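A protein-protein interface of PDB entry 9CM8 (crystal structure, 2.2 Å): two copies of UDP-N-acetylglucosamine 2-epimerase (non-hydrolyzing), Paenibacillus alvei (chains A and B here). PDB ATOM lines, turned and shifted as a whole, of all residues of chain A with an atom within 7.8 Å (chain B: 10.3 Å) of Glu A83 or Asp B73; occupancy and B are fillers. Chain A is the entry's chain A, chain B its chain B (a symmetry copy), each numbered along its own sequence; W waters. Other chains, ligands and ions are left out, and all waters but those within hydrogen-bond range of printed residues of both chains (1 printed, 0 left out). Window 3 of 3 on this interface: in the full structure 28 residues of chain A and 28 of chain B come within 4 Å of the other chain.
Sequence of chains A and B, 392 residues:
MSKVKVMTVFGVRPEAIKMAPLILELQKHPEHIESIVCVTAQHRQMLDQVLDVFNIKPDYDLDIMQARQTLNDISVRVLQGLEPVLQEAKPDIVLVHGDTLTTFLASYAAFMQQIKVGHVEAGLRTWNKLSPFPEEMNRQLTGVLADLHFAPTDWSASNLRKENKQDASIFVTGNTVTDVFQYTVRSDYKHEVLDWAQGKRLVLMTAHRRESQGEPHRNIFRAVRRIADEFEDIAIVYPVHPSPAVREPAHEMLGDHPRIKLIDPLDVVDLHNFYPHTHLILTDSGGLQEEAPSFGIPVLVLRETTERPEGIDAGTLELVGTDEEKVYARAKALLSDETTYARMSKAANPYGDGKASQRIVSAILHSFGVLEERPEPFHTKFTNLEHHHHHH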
ATOM      1  N   LEU A  62     -17.076  18.248   2.274  1.00  0.00           N
ATOM      2  CA  LEU A  62     -17.206  18.091   3.745  1.00  0.00           C
ATOM      3  C   LEU A  62     -18.248  16.986   3.946  1.00  0.00           C
ATOM      4  O   LEU A  62     -19.062  16.801   3.024  1.00  0.00           O
ATOM      5  CB  LEU A  62     -17.673  19.409   4.378  1.00  0.00           C
ATOM      6  CG  LEU A  62     -16.630  20.507   4.593  1.00  0.00           C
ATOM      7  CD1 LEU A  62     -15.767  20.741   3.366  1.00  0.00           C
ATOM      8  CD2 LEU A  62     -17.308  21.802   4.990  1.00  0.00           C
ATOM      9  N   ARG A  77     -19.385  21.971  13.089  1.00  0.00           N
ATOM     10  CA  ARG A  77     -18.780  21.017  12.117  1.00  0.00           C
ATOM     11  C   ARG A  77     -18.632  21.724  10.764  1.00  0.00           C
ATOM     12  O   ARG A  77     -17.547  21.585  10.157  1.00  0.00           O
ATOM     13  CB  ARG A  77     -19.565  19.691  12.073  1.00  0.00           C
ATOM     14  N   VAL A  78     -19.623  22.510  10.322  1.00  0.00           N
ATOM     15  CA  VAL A  78     -19.498  23.297   9.054  1.00  0.00           C
ATOM     16  C   VAL A  78     -18.347  24.277   9.215  1.00  0.00           C
ATOM     17  O   VAL A  78     -17.586  24.430   8.252  1.00  0.00           O
ATOM     18  CB  VAL A  78     -20.784  24.046   8.644  1.00  0.00           C
ATOM     19  CG1 VAL A  78     -20.514  25.044   7.517  1.00  0.00           C
ATOM     20  CG2 VAL A  78     -21.894  23.085   8.245  1.00  0.00           C
ATOM     21  N   LEU A  79     -18.233  24.960  10.362  1.00  0.00           N
ATOM     22  CA  LEU A  79     -17.171  25.999  10.537  1.00  0.00           C
ATOM     23  C   LEU A  79     -15.794  25.322  10.466  1.00  0.00           C
ATOM     24  O   LEU A  79     -14.927  25.828   9.736  1.00  0.00           O
ATOM     25  CB  LEU A  79     -17.342  26.763  11.859  1.00  0.00           C
ATOM     26  CG  LEU A  79     -18.001  28.150  11.785  1.00  0.00           C
ATOM     27  CD1 LEU A  79     -18.805  28.357  10.515  1.00  0.00           C
ATOM     28  CD2 LEU A  79     -18.871  28.406  13.006  1.00  0.00           C
ATOM     29  N   GLN A  80     -15.610  24.227  11.199  1.00  0.00           N
ATOM     30  CA  GLN A  80     -14.325  23.468  11.259  1.00  0.00           C
ATOM     31  C   GLN A  80     -13.918  23.013   9.846  1.00  0.00           C
ATOM     32  O   GLN A  80     -12.781  23.326   9.432  1.00  0.00           O
ATOM     33  CB  GLN A  80     -14.469  22.292  12.236  1.00  0.00           C
ATOM     34  CG  GLN A  80     -14.249  22.702  13.686  1.00  0.00           C
ATOM     35  CD  GLN A  80     -14.543  21.623  14.702  1.00  0.00           C
ATOM     36  OE1 GLN A  80     -14.045  21.664  15.825  1.00  0.00           O
ATOM     37  NE2 GLN A  80     -15.376  20.661  14.325  1.00  0.00           N
ATOM     38  N   GLY A  81     -14.831  22.358   9.122  1.00  0.00           N
ATOM     39  CA  GLY A  81     -14.609  21.834   7.757  1.00  0.00           C
ATOM     40  C   GLY A  81     -14.236  22.934   6.773  1.00  0.00           C
ATOM     41  O   GLY A  81     -13.265  22.750   5.998  1.00  0.00           O
ATOM     42  N   LEU A  82     -14.962  24.054   6.803  1.00  0.00           N
ATOM     43  CA  LEU A  82     -14.811  25.146   5.801  1.00  0.00           C
ATOM     44  C   LEU A  82     -13.510  25.919   6.006  1.00  0.00           C
ATOM     45  O   LEU A  82     -13.025  26.462   5.017  1.00  0.00           O
ATOM     46  CB  LEU A  82     -16.012  26.098   5.870  1.00  0.00           C
ATOM     47  CG  LEU A  82     -17.297  25.559   5.244  1.00  0.00           C
ATOM     48  CD1 LEU A  82     -18.377  26.643   5.191  1.00  0.00           C
ATOM     49  CD2 LEU A  82     -17.027  25.025   3.839  1.00  0.00           C
ATOM     50  N   GLU A  83     -13.005  26.049   7.235  1.00  0.00           N
ATOM     51  CA  GLU A  83     -11.792  26.878   7.475  1.00  0.00           C
ATOM     52  C   GLU A  83     -10.631  26.379   6.604  1.00  0.00           C
ATOM     53  O   GLU A  83     -10.009  27.166   5.895  1.00  0.00           O
ATOM     54  CB  GLU A  83     -11.382  26.926   8.951  1.00  0.00           C
ATOM     55  CG  GLU A  83      -9.938  27.368   9.121  1.00  0.00           C
ATOM     56  CD  GLU A  83      -9.576  27.967  10.463  1.00  0.00           C
ATOM     57  OE1 GLU A  83      -9.495  27.200  11.441  1.00  0.00           O
ATOM     58  OE2 GLU A  83      -9.377  29.195  10.519  1.00  0.00           O
ATOM     59  N   PRO A  84     -10.236  25.089   6.666  1.00  0.00           N
ATOM     60  CA  PRO A  84      -9.135  24.615   5.831  1.00  0.00           C
ATOM     61  C   PRO A  84      -9.486  24.736   4.337  1.00  0.00           C
ATOM     62  O   PRO A  84      -8.655  25.198   3.585  1.00  0.00           O
ATOM     63  CB  PRO A  84      -8.887  23.164   6.280  1.00  0.00           C
ATOM     64  CG  PRO A  84     -10.110  22.772   7.091  1.00  0.00           C
ATOM     65  CD  PRO A  84     -10.729  24.060   7.588  1.00  0.00           C
ATOM     66  N   VAL A  85     -10.696  24.356   3.926  1.00  0.00           N
ATOM     67  CA  VAL A  85     -11.100  24.528   2.504  1.00  0.00           C
ATOM     68  C   VAL A  85     -10.837  25.975   2.093  1.00  0.00           C
ATOM     69  O   VAL A  85     -10.242  26.143   1.034  1.00  0.00           O
ATOM     70  CB  VAL A  85     -12.548  24.116   2.198  1.00  0.00           C
ATOM     71  CG1 VAL A  85     -12.885  24.406   0.743  1.00  0.00           C
ATOM     72  CG2 VAL A  85     -12.816  22.660   2.517  1.00  0.00           C
ATOM     73  N   LEU A  86     -11.222  26.984   2.881  1.00  0.00           N
ATOM     74  CA  LEU A  86     -11.110  28.410   2.426  1.00  0.00           C
ATOM     75  C   LEU A  86      -9.646  28.862   2.397  1.00  0.00           C
ATOM     76  O   LEU A  86      -9.300  29.622   1.474  1.00  0.00           O
ATOM     77  CB  LEU A  86     -11.927  29.373   3.294  1.00  0.00           C
ATOM     78  CG  LEU A  86     -13.451  29.311   3.180  1.00  0.00           C
ATOM     79  CD1 LEU A  86     -14.076  30.324   4.130  1.00  0.00           C
ATOM     80  CD2 LEU A  86     -13.912  29.561   1.752  1.00  0.00           C
ATOM     81  N   GLN A  87      -8.810  28.483   3.370  1.00  0.00           N
ATOM     82  CA  GLN A  87      -7.395  28.969   3.373  1.00  0.00           C
ATOM     83  C   GLN A  87      -6.585  28.213   2.301  1.00  0.00           C
ATOM     84  O   GLN A  87      -5.609  28.799   1.835  1.00  0.00           O
ATOM     85  CB  GLN A  87      -6.768  29.007   4.782  1.00  0.00           C
ATOM     86  CG  GLN A  87      -6.688  27.678   5.527  1.00  0.00           C
ATOM     87  CD  GLN A  87      -6.653  27.826   7.037  1.00  0.00           C
ATOM     88  OE1 GLN A  87      -6.520  28.926   7.580  1.00  0.00           O
ATOM     89  NE2 GLN A  87      -6.794  26.710   7.741  1.00  0.00           N
ATOM     90  N   GLU A  88      -7.010  27.020   1.851  1.00  0.00           N
ATOM     91  CA  GLU A  88      -6.347  26.310   0.721  1.00  0.00           C
ATOM     92  C   GLU A  88      -6.760  26.952  -0.616  1.00  0.00           C
ATOM     93  O   GLU A  88      -5.868  27.372  -1.370  1.00  0.00           O
ATOM     94  CB  GLU A  88      -6.658  24.814   0.722  1.00  0.00           C
ATOM     95  CG  GLU A  88      -5.929  24.040  -0.372  1.00  0.00           C
ATOM     96  CD  GLU A  88      -6.074  22.524  -0.301  1.00  0.00           C
ATOM     97  OE1 GLU A  88      -7.058  21.995  -0.874  1.00  0.00           O
ATOM     98  OE2 GLU A  88      -5.201  21.869   0.334  1.00  0.00           O
ATOM     99  N   ALA A  89      -8.060  27.076  -0.889  1.00  0.00           N
ATOM    100  CA  ALA A  89      -8.583  27.536  -2.198  1.00  0.00           C
ATOM    101  C   ALA A  89      -8.468  29.059  -2.341  1.00  0.00           C
ATOM    102  O   ALA A  89      -8.350  29.536  -3.481  1.00  0.00           O
ATOM    103  CB  ALA A  89      -9.993  27.036  -2.373  1.00  0.00           C
ATOM    104  N   LYS A  90      -8.497  29.814  -1.248  1.00  0.00           N
ATOM    105  CA  LYS A  90      -8.505  31.308  -1.271  1.00  0.00           C
ATOM    106  C   LYS A  90      -9.403  31.843  -2.392  1.00  0.00           C
ATOM    107  O   LYS A  90      -8.960  32.582  -3.276  1.00  0.00           O
ATOM    108  CB  LYS A  90      -7.088  31.857  -1.444  1.00  0.00           C
ATOM    109  CG  LYS A  90      -6.091  31.449  -0.364  1.00  0.00           C
ATOM    110  CD  LYS A  90      -4.818  32.289  -0.393  1.00  0.00           C
ATOM    111  CE  LYS A  90      -3.588  31.558   0.112  1.00  0.00           C
ATOM    112  NZ  LYS A  90      -3.660  31.302   1.570  1.00  0.00           N
ATOM    113  N   ALA A 109     -18.088  31.776   7.733  1.00  0.00           N
ATOM    114  CA  ALA A 109     -16.714  31.246   7.508  1.00  0.00           C
ATOM    115  C   ALA A 109     -15.978  32.188   6.561  1.00  0.00           C
ATOM    116  O   ALA A 109     -14.802  32.483   6.830  1.00  0.00           O
ATOM    117  CB  ALA A 109     -16.760  29.844   6.976  1.00  0.00           C
ATOM    118  N   ALA A 110     -16.667  32.696   5.524  1.00  0.00           N
ATOM    119  CA  ALA A 110     -16.068  33.575   4.496  1.00  0.00           C
ATOM    120  C   ALA A 110     -15.798  34.949   5.111  1.00  0.00           C
ATOM    121  O   ALA A 110     -14.704  35.507   4.874  1.00  0.00           O
ATOM    122  CB  ALA A 110     -16.970  33.657   3.288  1.00  0.00           C
ATOM    123  N   MET A 112     -15.082  35.586   8.140  1.00  0.00           N
ATOM    124  CA  MET A 112     -13.940  35.464   9.082  1.00  0.00           C
ATOM    125  C   MET A 112     -12.606  35.256   8.352  1.00  0.00           C
ATOM    126  O   MET A 112     -11.591  35.193   9.054  1.00  0.00           O
ATOM    127  CB  MET A 112     -14.180  34.332  10.075  1.00  0.00           C
ATOM    128  CG  MET A 112     -15.215  34.743  11.094  1.00  0.00           C
ATOM    129  SD  MET A 112     -15.301  33.547  12.397  1.00  0.00           S
ATOM    130  CE  MET A 112     -15.666  32.107  11.399  1.00  0.00           C
ATOM    131  N   GLN A 113     -12.593  35.212   7.014  1.00  0.00           N
ATOM    132  CA  GLN A 113     -11.346  35.260   6.213  1.00  0.00           C
ATOM    133  C   GLN A 113     -11.408  36.448   5.252  1.00  0.00           C
ATOM    134  O   GLN A 113     -10.612  36.490   4.337  1.00  0.00           O
ATOM    135  CB  GLN A 113     -11.139  33.894   5.566  1.00  0.00           C
ATOM    136  CG  GLN A 113     -11.079  32.780   6.600  1.00  0.00           C
ATOM    137  CD  GLN A 113     -10.415  31.520   6.114  1.00  0.00           C
ATOM    138  OE1 GLN A 113      -9.432  31.546   5.367  1.00  0.00           O
ATOM    139  NE2 GLN A 113     -10.947  30.392   6.555  1.00  0.00           N
ATOM    140  N   ILE A 115     -13.367  37.172   2.923  1.00  0.00           N
ATOM    141  CA  ILE A 115     -13.737  36.756   1.542  1.00  0.00           C
ATOM    142  C   ILE A 115     -15.147  37.281   1.228  1.00  0.00           C
ATOM    143  O   ILE A 115     -16.048  37.032   2.018  1.00  0.00           O
ATOM    144  CB  ILE A 115     -13.600  35.233   1.403  1.00  0.00           C
ATOM    145  CG1 ILE A 115     -12.140  34.804   1.623  1.00  0.00           C
ATOM    146  CG2 ILE A 115     -14.148  34.743   0.068  1.00  0.00           C
ATOM    147  CD1 ILE A 115     -11.955  33.312   1.858  1.00  0.00           C
ATOM    148  N   GLN B  42     -10.914  35.477  26.532  1.00  0.00           N
ATOM    149  CA  GLN B  42      -9.632  35.062  25.877  1.00  0.00           C
ATOM    150  C   GLN B  42      -8.454  35.863  26.461  1.00  0.00           C
ATOM    151  O   GLN B  42      -8.271  35.833  27.699  1.00  0.00           O
ATOM    152  CB  GLN B  42      -9.702  35.273  24.359  1.00  0.00           C
ATOM    153  N   LEU B  62     -15.981  29.823  30.574  1.00  0.00           N
ATOM    154  CA  LEU B  62     -15.255  29.043  29.533  1.00  0.00           C
ATOM    155  C   LEU B  62     -13.856  29.647  29.373  1.00  0.00           C
ATOM    156  O   LEU B  62     -13.775  30.817  28.978  1.00  0.00           O
ATOM    157  CB  LEU B  62     -16.027  29.036  28.208  1.00  0.00           C
ATOM    158  CG  LEU B  62     -17.349  29.800  28.152  1.00  0.00           C
ATOM    159  CD1 LEU B  62     -17.814  29.957  26.710  1.00  0.00           C
ATOM    160  CD2 LEU B  62     -18.424  29.103  28.970  1.00  0.00           C
ATOM    161  N   ILE B  64     -11.327  30.229  27.532  1.00  0.00           N
ATOM    162  CA  ILE B  64     -11.050  30.226  26.056  1.00  0.00           C
ATOM    163  C   ILE B  64      -9.558  30.507  25.790  1.00  0.00           C
ATOM    164  O   ILE B  64      -9.049  31.505  26.328  1.00  0.00           O
ATOM    165  CB  ILE B  64     -11.959  31.241  25.319  1.00  0.00           C
ATOM    166  CG1 ILE B  64     -13.450  31.013  25.584  1.00  0.00           C
ATOM    167  CG2 ILE B  64     -11.660  31.252  23.826  1.00  0.00           C
ATOM    168  CD1 ILE B  64     -13.961  29.652  25.171  1.00  0.00           C
ATOM    169  N   MET B  65      -8.922  29.698  24.925  1.00  0.00           N
ATOM    170  CA  MET B  65      -7.440  29.569  24.741  1.00  0.00           C
ATOM    171  C   MET B  65      -6.788  30.946  24.527  1.00  0.00           C
ATOM    172  O   MET B  65      -7.471  31.830  23.974  1.00  0.00           O
ATOM    173  CB  MET B  65      -7.116  28.642  23.558  1.00  0.00           C
ATOM    174  CG  MET B  65      -5.646  28.655  23.108  1.00  0.00           C
ATOM    175  SD  MET B  65      -5.104  27.136  22.225  1.00  0.00           S
ATOM    176  CE  MET B  65      -3.540  27.688  21.542  1.00  0.00           C
ATOM    177  N   GLN B  69      -5.166  32.317  17.909  1.00  0.00           N
ATOM    178  CA  GLN B  69      -6.657  32.220  17.929  1.00  0.00           C
ATOM    179  C   GLN B  69      -7.271  33.091  16.814  1.00  0.00           C
ATOM    180  O   GLN B  69      -7.336  34.336  16.979  1.00  0.00           O
ATOM    181  CB  GLN B  69      -7.189  32.626  19.307  1.00  0.00           C
ATOM    182  N   THR B  70      -7.705  32.462  15.716  1.00  0.00           N
ATOM    183  CA  THR B  70      -8.478  33.107  14.625  1.00  0.00           C
ATOM    184  C   THR B  70      -9.846  33.489  15.192  1.00  0.00           C
ATOM    185  O   THR B  70     -10.172  33.073  16.340  1.00  0.00           O
ATOM    186  CB  THR B  70      -8.597  32.213  13.376  1.00  0.00           C
ATOM    187  OG1 THR B  70      -9.259  30.993  13.698  1.00  0.00           O
ATOM    188  CG2 THR B  70      -7.263  31.864  12.750  1.00  0.00           C
ATOM    189  N   LEU B  71     -10.613  34.268  14.431  1.00  0.00           N
ATOM    190  CA  LEU B  71     -12.040  34.504  14.733  1.00  0.00           C
ATOM    191  C   LEU B  71     -12.779  33.160  14.688  1.00  0.00           C
ATOM    192  O   LEU B  71     -13.668  32.947  15.526  1.00  0.00           O
ATOM    193  CB  LEU B  71     -12.590  35.539  13.746  1.00  0.00           C
ATOM    194  CG  LEU B  71     -11.986  36.934  13.903  1.00  0.00           C
ATOM    195  CD1 LEU B  71     -12.457  37.852  12.801  1.00  0.00           C
ATOM    196  CD2 LEU B  71     -12.298  37.525  15.268  1.00  0.00           C
ATOM    197  N   ASN B  72     -12.397  32.267  13.778  1.00  0.00           N
ATOM    198  CA  ASN B  72     -13.042  30.941  13.592  1.00  0.00           C
ATOM    199  C   ASN B  72     -12.832  30.041  14.832  1.00  0.00           C
ATOM    200  O   ASN B  72     -13.786  29.353  15.213  1.00  0.00           O
ATOM    201  CB  ASN B  72     -12.560  30.282  12.297  1.00  0.00           C
ATOM    202  CG  ASN B  72     -13.467  29.158  11.845  1.00  0.00           C
ATOM    203  OD1 ASN B  72     -14.259  29.324  10.919  1.00  0.00           O
ATOM    204  ND2 ASN B  72     -13.349  28.001  12.474  1.00  0.00           N
ATOM    205  N   ASP B  73     -11.629  30.021  15.420  1.00  0.00           N
ATOM    206  CA  ASP B  73     -11.277  29.223  16.631  1.00  0.00           C
ATOM    207  C   ASP B  73     -12.155  29.683  17.792  1.00  0.00           C
ATOM    208  O   ASP B  73     -12.888  28.843  18.313  1.00  0.00           O
ATOM    209  CB  ASP B  73      -9.805  29.385  17.025  1.00  0.00           C
ATOM    210  CG  ASP B  73      -8.801  28.893  15.991  1.00  0.00           C
ATOM    211  OD1 ASP B  73      -9.099  27.894  15.322  1.00  0.00           O
ATOM    212  OD2 ASP B  73      -7.720  29.517  15.878  1.00  0.00           O
ATOM    213  N   ILE B  74     -12.079  30.974  18.149  1.00  0.00           N
ATOM    214  CA  ILE B  74     -12.977  31.627  19.142  1.00  0.00           C
ATOM    215  C   ILE B  74     -14.417  31.180  18.857  1.00  0.00           C
ATOM    216  O   ILE B  74     -15.079  30.649  19.772  1.00  0.00           O
ATOM    217  CB  ILE B  74     -12.823  33.159  19.104  1.00  0.00           C
ATOM    218  CG1 ILE B  74     -11.454  33.593  19.629  1.00  0.00           C
ATOM    219  CG2 ILE B  74     -13.929  33.845  19.876  1.00  0.00           C
ATOM    220  CD1 ILE B  74     -10.994  34.932  19.100  1.00  0.00           C
ATOM    221  N   SER B  75     -14.866  31.354  17.614  1.00  0.00           N
ATOM    222  CA  SER B  75     -16.251  31.070  17.195  1.00  0.00           C
ATOM    223  C   SER B  75     -16.591  29.640  17.580  1.00  0.00           C
ATOM    224  O   SER B  75     -17.574  29.460  18.334  1.00  0.00           O
ATOM    225  CB  SER B  75     -16.462  31.355  15.739  1.00  0.00           C
ATOM    226  OG  SER B  75     -16.265  32.742  15.498  1.00  0.00           O
ATOM    227  N   VAL B  76     -15.782  28.663  17.153  1.00  0.00           N
ATOM    228  CA  VAL B  76     -16.039  27.223  17.472  1.00  0.00           C
ATOM    229  C   VAL B  76     -15.992  27.030  18.994  1.00  0.00           C
ATOM    230  O   VAL B  76     -16.911  26.368  19.525  1.00  0.00           O
ATOM    231  CB  VAL B  76     -15.058  26.276  16.753  1.00  0.00           C
ATOM    232  CG1 VAL B  76     -15.131  24.864  17.320  1.00  0.00           C
ATOM    233  CG2 VAL B  76     -15.294  26.265  15.249  1.00  0.00           C
ATOM    234  N   ARG B  77     -15.003  27.614  19.680  1.00  0.00           N
ATOM    235  CA  ARG B  77     -14.805  27.351  21.132  1.00  0.00           C
ATOM    236  C   ARG B  77     -16.022  27.847  21.915  1.00  0.00           C
ATOM    237  O   ARG B  77     -16.607  27.002  22.627  1.00  0.00           O
ATOM    238  CB  ARG B  77     -13.489  27.911  21.679  1.00  0.00           C
ATOM    239  CG  ARG B  77     -12.315  26.949  21.528  1.00  0.00           C
ATOM    240  CD  ARG B  77     -11.005  27.547  22.018  1.00  0.00           C
ATOM    241  NE  ARG B  77      -9.893  26.603  21.922  1.00  0.00           N
ATOM    242  CZ  ARG B  77      -9.087  26.446  20.867  1.00  0.00           C
ATOM    243  NH1 ARG B  77      -9.241  27.177  19.773  1.00  0.00           N
ATOM    244  NH2 ARG B  77      -8.115  25.548  20.919  1.00  0.00           N
ATOM    245  N   VAL B  78     -16.417  29.122  21.745  1.00  0.00           N
ATOM    246  CA  VAL B  78     -17.571  29.733  22.475  1.00  0.00           C
ATOM    247  C   VAL B  78     -18.830  28.889  22.218  1.00  0.00           C
ATOM    248  O   VAL B  78     -19.542  28.599  23.183  1.00  0.00           O
ATOM    249  CB  VAL B  78     -17.804  31.213  22.103  1.00  0.00           C
ATOM    250  CG1 VAL B  78     -19.015  31.786  22.826  1.00  0.00           C
ATOM    251  CG2 VAL B  78     -16.587  32.074  22.378  1.00  0.00           C
ATOM    252  N   LEU B  79     -19.132  28.524  20.975  1.00  0.00           N
ATOM    253  CA  LEU B  79     -20.340  27.714  20.650  1.00  0.00           C
ATOM    254  C   LEU B  79     -20.306  26.380  21.416  1.00  0.00           C
ATOM    255  O   LEU B  79     -21.315  26.056  22.076  1.00  0.00           O
ATOM    256  CB  LEU B  79     -20.403  27.485  19.144  1.00  0.00           C
ATOM    257  CG  LEU B  79     -21.402  28.334  18.359  1.00  0.00           C
ATOM    258  CD1 LEU B  79     -21.785  29.618  19.075  1.00  0.00           C
ATOM    259  CD2 LEU B  79     -20.859  28.637  16.977  1.00  0.00           C
ATOM    260  N   GLN B  80     -19.184  25.657  21.347  1.00  0.00           N
ATOM    261  CA  GLN B  80     -18.947  24.373  22.072  1.00  0.00           C
ATOM    262  C   GLN B  80     -19.134  24.574  23.579  1.00  0.00           C
ATOM    263  O   GLN B  80     -19.861  23.780  24.161  1.00  0.00           O
ATOM    264  CB  GLN B  80     -17.548  23.813  21.785  1.00  0.00           C
ATOM    265  CG  GLN B  80     -17.503  22.946  20.542  1.00  0.00           C
ATOM    266  CD  GLN B  80     -16.108  22.516  20.151  1.00  0.00           C
ATOM    267  OE1 GLN B  80     -15.110  23.196  20.403  1.00  0.00           O
ATOM    268  NE2 GLN B  80     -16.039  21.383  19.481  1.00  0.00           N
ATOM    269  N   GLY B  81     -18.513  25.604  24.167  1.00  0.00           N
ATOM    270  CA  GLY B  81     -18.621  25.945  25.601  1.00  0.00           C
ATOM    271  C   GLY B  81     -20.050  26.258  26.046  1.00  0.00           C
ATOM    272  O   GLY B  81     -20.444  25.845  27.167  1.00  0.00           O
ATOM    273  N   LEU B 101     -17.257  39.783  19.261  1.00  0.00           N
ATOM    274  CA  LEU B 101     -17.589  38.532  18.517  1.00  0.00           C
ATOM    275  C   LEU B 101     -18.424  37.644  19.438  1.00  0.00           C
ATOM    276  O   LEU B 101     -19.369  36.944  18.975  1.00  0.00           O
ATOM    277  CB  LEU B 101     -16.285  37.822  18.130  1.00  0.00           C
ATOM    278  CG  LEU B 101     -16.159  37.324  16.693  1.00  0.00           C
ATOM    279  CD1 LEU B 101     -15.231  36.119  16.645  1.00  0.00           C
ATOM    280  CD2 LEU B 101     -17.500  36.974  16.065  1.00  0.00           C
ATOM    281  N   THR B 102     -18.069  37.673  20.717  1.00  0.00           N
ATOM    282  CA  THR B 102     -18.663  36.842  21.798  1.00  0.00           C
ATOM    283  C   THR B 102     -20.147  37.201  22.011  1.00  0.00           C
ATOM    284  O   THR B 102     -20.971  36.286  22.214  1.00  0.00           O
ATOM    285  CB  THR B 102     -17.819  37.023  23.065  1.00  0.00           C
ATOM    286  OG1 THR B 102     -16.638  36.266  22.809  1.00  0.00           O
ATOM    287  CG2 THR B 102     -18.498  36.529  24.315  1.00  0.00           C
ATOM    288  N   LEU B 105     -21.797  35.477  19.165  1.00  0.00           N
ATOM    289  CA  LEU B 105     -21.743  33.992  19.349  1.00  0.00           C
ATOM    290  C   LEU B 105     -22.757  33.569  20.425  1.00  0.00           C
ATOM    291  O   LEU B 105     -23.470  32.550  20.208  1.00  0.00           O
ATOM    292  CB  LEU B 105     -20.325  33.563  19.753  1.00  0.00           C
ATOM    293  CG  LEU B 105     -19.331  33.228  18.641  1.00  0.00           C
ATOM    294  CD1 LEU B 105     -19.964  33.083  17.281  1.00  0.00           C
ATOM    295  CD2 LEU B 105     -18.221  34.231  18.605  1.00  0.00           C
HETATM  296  O   HOH W   1     -13.369  30.453   8.129  1.00  0.00           O
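The side-chain hydroxyl of Ser B75 is in hydrogen-bond range of the side-chain sulfur of Met A112, at 3.3 Å. SD of Met A112 is in hydrogen-bond range of N of Asn B72, 3.5 Å away. The side-chain sulfur (SD) of Met A112 lies close to the backbone carbonyl oxygen (O) of Leu B71.
The backbone carbonyl oxygen of Glu A83 is in hydrogen-bond range of the side-chain amide nitrogen of Gln A113, at 3.4 Å. N of Thr B70 lies within hydrogen-bond range of OD2 of Asp B73, at 2.9 Å. The backbone carbonyl oxygen of Leu B71 sits at hydrogen-bond distance from the side-chain hydroxyl of Ser B75. The backbone NH (N) of Asn B72 sits close to the side-chain hydroxyl (OG1) of Thr B70, 3.4 Å away.
Among the printed residues, pairs that only touch across the chains: Glu A83 with Thr B70 (3.7 Å), Gln A80 with Val B76 (3.7 Å), Leu A79 with Asn B72 (3.8 Å), Glu A83 with Asn B72 (3.8 Å), Glu A83 with Asp B73 (3.96 Å) and Leu A79 with Val B76 (3.99 Å).
Arg A77 touches none of the printed residues of chain B. Printed residues of chain B within 4 Å of Gln A80: Val B76 (3.7 Å). No residue of chain B comes within 4 Å of Leu A82. Glu A83 touches just these residues of chain B: Thr B70 (3.7 Å), Asn B72 (3.8 Å) and Asp B73 (3.96 Å). No residue of chain B comes within 4 Å of Leu A86. Asp B73 touches just one residue of chain A: Glu A83 (3.96 Å). Of the printed residues of chain A, Ser B75 touches Met A112. Of the printed residues of chain A, Val B76 touches Leu A79 (3.99 Å) and Gln A80 (3.7 Å). The nearest residue of chain B that does not touch Glu A83 is Leu B71 (6.5 Å). The nearest residue of chain A that does not touch Asp B73 is Met A112 (5.9 Å).
Hydrophobic or aromatic side chains of chain A that line the printed part of chain B: Leu A79 and Met A112. Among the printed residues, 9 pairs touch across the chains. Among the printed residues, no Asp or Glu carboxylate lies within 4 Å of a Lys or Arg side-chain nitrogen of the other chain.
6 positions are printed for both chains. Of the 9 pairs that touch across the chains among the printed residues, none has its exchanged pair printed and touching as well.
Water W1 lies within hydrogen-bond range of the backbone carbonyl oxygen (O) of Ala A109 (2.8 Å), the side-chain amide nitrogen (NE2) of Gln A113 (2.9 Å) and the side-chain amide oxygen (OD1) of Asn B72 (3.1 Å).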
